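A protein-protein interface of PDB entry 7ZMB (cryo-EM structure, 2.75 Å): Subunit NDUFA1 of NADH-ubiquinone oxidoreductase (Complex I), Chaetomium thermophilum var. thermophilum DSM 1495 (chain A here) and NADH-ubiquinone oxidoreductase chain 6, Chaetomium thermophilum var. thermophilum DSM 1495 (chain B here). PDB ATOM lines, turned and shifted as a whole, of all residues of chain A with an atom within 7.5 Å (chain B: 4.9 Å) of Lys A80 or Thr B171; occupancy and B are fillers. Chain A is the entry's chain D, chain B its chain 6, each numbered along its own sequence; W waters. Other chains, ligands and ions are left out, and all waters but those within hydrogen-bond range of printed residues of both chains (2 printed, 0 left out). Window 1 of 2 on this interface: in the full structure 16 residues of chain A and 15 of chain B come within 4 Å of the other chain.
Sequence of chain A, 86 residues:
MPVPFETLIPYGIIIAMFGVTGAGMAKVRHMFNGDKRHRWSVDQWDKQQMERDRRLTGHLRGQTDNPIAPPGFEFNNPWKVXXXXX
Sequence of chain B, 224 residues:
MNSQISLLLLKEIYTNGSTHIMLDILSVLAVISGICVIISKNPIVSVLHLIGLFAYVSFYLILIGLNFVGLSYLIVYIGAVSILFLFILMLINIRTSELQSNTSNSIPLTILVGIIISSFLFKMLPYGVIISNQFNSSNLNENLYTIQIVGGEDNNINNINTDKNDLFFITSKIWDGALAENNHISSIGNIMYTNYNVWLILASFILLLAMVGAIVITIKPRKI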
ATOM      1  N   GLU A  51      16.454  27.003  25.386  1.00  0.00           N
ATOM      2  CA  GLU A  51      17.869  27.397  25.225  1.00  0.00           C
ATOM      3  C   GLU A  51      17.888  28.563  24.244  1.00  0.00           C
ATOM      4  O   GLU A  51      18.771  29.418  24.376  1.00  0.00           O
ATOM      5  CB  GLU A  51      18.671  26.229  24.668  1.00  0.00           C
ATOM      6  CG  GLU A  51      18.949  25.138  25.679  1.00  0.00           C
ATOM      7  CD  GLU A  51      19.415  23.848  25.029  1.00  0.00           C
ATOM      8  OE1 GLU A  51      19.034  23.610  23.867  1.00  0.00           O
ATOM      9  OE2 GLU A  51      20.167  23.096  25.678  1.00  0.00           O
ATOM     10  N   ARG A  54      17.311  31.674  26.358  1.00  0.00           N
ATOM     11  CA  ARG A  54      18.579  32.105  26.997  1.00  0.00           C
ATOM     12  C   ARG A  54      19.417  32.867  25.972  1.00  0.00           C
ATOM     13  O   ARG A  54      20.042  33.854  26.357  1.00  0.00           O
ATOM     14  CB  ARG A  54      19.311  30.884  27.545  1.00  0.00           C
ATOM     15  CG  ARG A  54      20.393  31.205  28.563  1.00  0.00           C
ATOM     16  CD  ARG A  54      21.412  30.089  28.631  1.00  0.00           C
ATOM     17  NE  ARG A  54      21.116  29.060  29.613  1.00  0.00           N
ATOM     18  CZ  ARG A  54      21.676  27.861  29.619  1.00  0.00           C
ATOM     19  NH1 ARG A  54      21.369  26.988  30.561  1.00  0.00           N
ATOM     20  NH2 ARG A  54      22.537  27.536  28.673  1.00  0.00           N
ATOM     21  N   ASN A  77      24.802  30.757  19.383  1.00  0.00           N
ATOM     22  CA  ASN A  77      24.085  29.453  19.283  1.00  0.00           C
ATOM     23  C   ASN A  77      24.972  28.406  19.940  1.00  0.00           C
ATOM     24  O   ASN A  77      26.068  28.165  19.426  1.00  0.00           O
ATOM     25  CB  ASN A  77      23.715  29.070  17.850  1.00  0.00           C
ATOM     26  CG  ASN A  77      22.752  27.907  17.763  1.00  0.00           C
ATOM     27  OD1 ASN A  77      22.022  27.621  18.708  1.00  0.00           O
ATOM     28  ND2 ASN A  77      22.728  27.237  16.622  1.00  0.00           N
ATOM     29  N   PRO A  78      24.555  27.766  21.049  1.00  0.00           N
ATOM     30  CA  PRO A  78      25.454  26.865  21.757  1.00  0.00           C
ATOM     31  C   PRO A  78      25.705  25.525  21.058  1.00  0.00           C
ATOM     32  O   PRO A  78      24.761  24.954  20.577  1.00  0.00           O
ATOM     33  CB  PRO A  78      24.705  26.651  23.080  1.00  0.00           C
ATOM     34  CG  PRO A  78      23.250  26.773  22.702  1.00  0.00           C
ATOM     35  CD  PRO A  78      23.230  27.870  21.660  1.00  0.00           C
ATOM     36  N   TRP A  79      26.959  25.093  20.975  1.00  0.00           N
ATOM     37  CA  TRP A  79      27.246  23.729  20.461  1.00  0.00           C
ATOM     38  C   TRP A  79      27.727  22.942  21.676  1.00  0.00           C
ATOM     39  O   TRP A  79      28.678  23.395  22.311  1.00  0.00           O
ATOM     40  CB  TRP A  79      28.226  23.740  19.289  1.00  0.00           C
ATOM     41  CG  TRP A  79      27.569  23.868  17.949  1.00  0.00           C
ATOM     42  CD1 TRP A  79      26.316  24.333  17.684  1.00  0.00           C
ATOM     43  CD2 TRP A  79      28.146  23.530  16.675  1.00  0.00           C
ATOM     44  NE1 TRP A  79      26.068  24.303  16.340  1.00  0.00           N
ATOM     45  CE2 TRP A  79      27.173  23.817  15.694  1.00  0.00           C
ATOM     46  CE3 TRP A  79      29.382  23.017  16.268  1.00  0.00           C
ATOM     47  CZ2 TRP A  79      27.402  23.606  14.336  1.00  0.00           C
ATOM     48  CZ3 TRP A  79      29.606  22.805  14.926  1.00  0.00           C
ATOM     49  CH2 TRP A  79      28.629  23.099  13.975  1.00  0.00           C
ATOM     50  N   LYS A  80      27.111  21.809  21.981  1.00  0.00           N
ATOM     51  CA  LYS A  80      27.394  21.125  23.232  1.00  0.00           C
ATOM     52  C   LYS A  80      28.636  20.249  23.094  1.00  0.00           C
ATOM     53  O   LYS A  80      28.821  19.564  22.089  1.00  0.00           O
ATOM     54  CB  LYS A  80      26.191  20.278  23.633  1.00  0.00           C
ATOM     55  CG  LYS A  80      24.939  21.094  23.812  1.00  0.00           C
ATOM     56  CD  LYS A  80      25.029  22.041  24.946  1.00  0.00           C
ATOM     57  CE  LYS A  80      23.695  22.713  25.169  1.00  0.00           C
ATOM     58  NZ  LYS A  80      23.376  23.636  24.054  1.00  0.00           N
ATOM     59  N   VAL A  81      29.506  20.257  24.106  1.00  0.00           N
ATOM     60  CA  VAL A  81      30.777  19.467  24.065  1.00  0.00           C
ATOM     61  C   VAL A  81      30.760  18.391  25.156  1.00  0.00           C
ATOM     62  O   VAL A  81      30.482  18.736  26.313  1.00  0.00           O
ATOM     63  CB  VAL A  81      32.010  20.383  24.192  1.00  0.00           C
ATOM     64  CG1 VAL A  81      33.270  19.624  24.565  1.00  0.00           C
ATOM     65  CG2 VAL A  81      32.235  21.229  22.951  1.00  0.00           C
ATOM     66  N   UNK A  82      31.028  17.133  24.791  1.00  0.00           N
ATOM     67  CA  UNK A  82      31.062  16.014  25.762  1.00  0.00           C
ATOM     68  C   UNK A  82      32.345  15.202  25.578  1.00  0.00           C
ATOM     69  O   UNK A  82      32.809  15.089  24.439  1.00  0.00           O
ATOM     70  CB  UNK A  82      29.842  15.139  25.599  1.00  0.00           C
ATOM     71  N   UNK A  85      29.894  10.301  26.040  1.00  0.00           N
ATOM     72  CA  UNK A  85      28.667   9.623  25.529  1.00  0.00           C
ATOM     73  C   UNK A  85      28.078  10.132  24.225  1.00  0.00           C
ATOM     74  O   UNK A  85      27.069  10.840  24.270  1.00  0.00           O
ATOM     75  CB  UNK A  85      27.620   9.432  26.580  1.00  0.00           C
ATOM     76  N   UNK A  86      28.668   9.716  23.112  1.00  0.00           N
ATOM     77  CA  UNK A  86      28.076  10.011  21.799  1.00  0.00           C
ATOM     78  C   UNK A  86      26.921   9.024  21.590  1.00  0.00           C
ATOM     79  O   UNK A  86      26.919   7.992  22.291  1.00  0.00           O
ATOM     80  CB  UNK A  86      29.123   9.868  20.732  1.00  0.00           C
ATOM     81  N   GLU B  12      29.050  25.004  30.681  1.00  0.00           N
ATOM     82  CA  GLU B  12      27.568  25.086  30.641  1.00  0.00           C
ATOM     83  C   GLU B  12      27.028  25.346  32.054  1.00  0.00           C
ATOM     84  O   GLU B  12      27.319  24.544  32.948  1.00  0.00           O
ATOM     85  CB  GLU B  12      27.036  23.769  30.092  1.00  0.00           C
ATOM     86  CG  GLU B  12      25.713  23.901  29.367  1.00  0.00           C
ATOM     87  CD  GLU B  12      25.341  22.651  28.591  1.00  0.00           C
ATOM     88  OE1 GLU B  12      26.233  21.814  28.370  1.00  0.00           O
ATOM     89  OE2 GLU B  12      24.164  22.514  28.227  1.00  0.00           O
ATOM     90  N   PHE B 169      33.183  15.170  21.541  1.00  0.00           N
ATOM     91  CA  PHE B 169      31.994  15.005  20.675  1.00  0.00           C
ATOM     92  C   PHE B 169      31.222  16.320  20.687  1.00  0.00           C
ATOM     93  O   PHE B 169      31.096  16.932  21.754  1.00  0.00           O
ATOM     94  CB  PHE B 169      31.169  13.799  21.128  1.00  0.00           C
ATOM     95  CG  PHE B 169      31.875  12.469  21.110  1.00  0.00           C
ATOM     96  CD1 PHE B 169      31.886  11.687  19.968  1.00  0.00           C
ATOM     97  CD2 PHE B 169      32.508  11.987  22.243  1.00  0.00           C
ATOM     98  CE1 PHE B 169      32.519  10.455  19.958  1.00  0.00           C
ATOM     99  CE2 PHE B 169      33.149  10.758  22.228  1.00  0.00           C
ATOM    100  CZ  PHE B 169      33.155   9.996  21.086  1.00  0.00           C
ATOM    101  N   ILE B 170      30.747  16.746  19.519  1.00  0.00           N
ATOM    102  CA  ILE B 170      29.999  18.029  19.414  1.00  0.00           C
ATOM    103  C   ILE B 170      28.557  17.723  19.003  1.00  0.00           C
ATOM    104  O   ILE B 170      28.360  16.912  18.088  1.00  0.00           O
ATOM    105  CB  ILE B 170      30.722  19.007  18.468  1.00  0.00           C
ATOM    106  CG1 ILE B 170      30.155  20.424  18.558  1.00  0.00           C
ATOM    107  CG2 ILE B 170      30.790  18.495  17.039  1.00  0.00           C
ATOM    108  CD1 ILE B 170      30.655  21.194  19.749  1.00  0.00           C
ATOM    109  N   THR B 171      27.589  18.311  19.704  1.00  0.00           N
ATOM    110  CA  THR B 171      26.159  18.100  19.357  1.00  0.00           C
ATOM    111  C   THR B 171      25.461  19.447  19.142  1.00  0.00           C
ATOM    112  O   THR B 171      25.866  20.425  19.769  1.00  0.00           O
ATOM    113  CB  THR B 171      25.443  17.219  20.387  1.00  0.00           C
ATOM    114  OG1 THR B 171      25.280  17.947  21.604  1.00  0.00           O
ATOM    115  CG2 THR B 171      26.153  15.912  20.646  1.00  0.00           C
ATOM    116  N   SER B 172      24.504  19.492  18.221  1.00  0.00           N
ATOM    117  CA  SER B 172      23.714  20.725  17.980  1.00  0.00           C
ATOM    118  C   SER B 172      22.228  20.358  17.947  1.00  0.00           C
ATOM    119  O   SER B 172      21.893  19.263  18.411  1.00  0.00           O
ATOM    120  CB  SER B 172      24.132  21.396  16.711  1.00  0.00           C
ATOM    121  OG  SER B 172      23.853  20.568  15.600  1.00  0.00           O
ATOM    122  N   LYS B 173      21.380  21.211  17.386  1.00  0.00           N
ATOM    123  CA  LYS B 173      19.926  20.940  17.425  1.00  0.00           C
ATOM    124  C   LYS B 173      19.314  20.957  16.026  1.00  0.00           C
ATOM    125  O   LYS B 173      19.882  21.625  15.161  1.00  0.00           O
ATOM    126  CB  LYS B 173      19.286  21.993  18.330  1.00  0.00           C
ATOM    127  CG  LYS B 173      19.267  23.413  17.788  1.00  0.00           C
ATOM    128  CD  LYS B 173      18.552  24.386  18.686  1.00  0.00           C
ATOM    129  CE  LYS B 173      19.216  24.566  20.032  1.00  0.00           C
ATOM    130  NZ  LYS B 173      18.494  25.562  20.859  1.00  0.00           N
HETATM  131  O   HOH W   1      22.741  23.992  18.115  1.00  0.00           O
HETATM  132  O   HOH W   2      27.634  17.097  23.433  1.00  0.00           O
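Water W2 bridges O of Lys A80 (3.0 Å) and OG1 of Thr B171 (3.1 Å).
Water W1 bridges the backbone NH (N) of Lys B173 (3.2 Å) and the backbone carbonyl oxygen (O) of Pro A78 (3.3 Å).
Among the printed residues, merely in contact across the chains: Lys A80 with Glu B12 (3.1 Å), Lys A80 with Ile B170 (3.3 Å), UNK A86 with Phe B169 (3.4 Å), Val A81 with Phe B169 (3.4 Å), Trp A79 with Ser B172 (3.5 Å), Trp A79 with Ile B170 (3.5 Å), Val A81 with Ile B170 (3.6 Å) and Trp A79 with Thr B171 (3.6 Å).
Of chain B, only Glu B12, Phe B169, Ile B170 and Thr B171 come within 4 Å of Lys A80.
Thr B171 touches just these residues of chain A: Trp A79 (3.6 Å) and Lys A80 (2.9 Å).
Printed residues of chain B within 4 Å of Val A81: Phe B169 and Ile B170.
Of the printed residues of chain A, Phe B169 touches Lys A80, Val A81, UNK A82 and UNK A86.
Of the printed residues of chain B, UNK A86 touches Phe B169.
The nearest printed residue of chain B that does not touch Lys A80 is Ser B172 (5.1 Å).
The backbone NH (N) of Lys A80 is in hydrogen-bond range of the backbone carbonyl oxygen (O) of Thr B171 (2.9 Å).
NZ of Lys B173 lies within salt-bridge range of OE1 of Glu A51, at 3.6 Å.
O of UNK A82 lies within hydrogen-bond range of the backbone NH (N) of Phe B169.
The backbone carbonyl oxygen (O) of Lys A80 lies close to the backbone carbonyl oxygen (O) of Phe B169.
OE2 of Glu A51 lies within salt-bridge range of NZ of Lys A80.
Along chain A the printed residues that touch a printed residue of chain B span positions 51 to 86.
Of the 6 printed residues of chain B, 6 touch a printed residue of chain A.
Hydrophobic or aromatic side chains of chain B within 4 Å of the printed part of chain A: Phe B169 and Ile B170.
Among the printed residues, 12 pairs touch across the chains.
Among the printed residues, Asp or Glu carboxylates within 4 Å of a Lys or Arg side-chain nitrogen of the other chain: Glu A51 with Lys B173.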
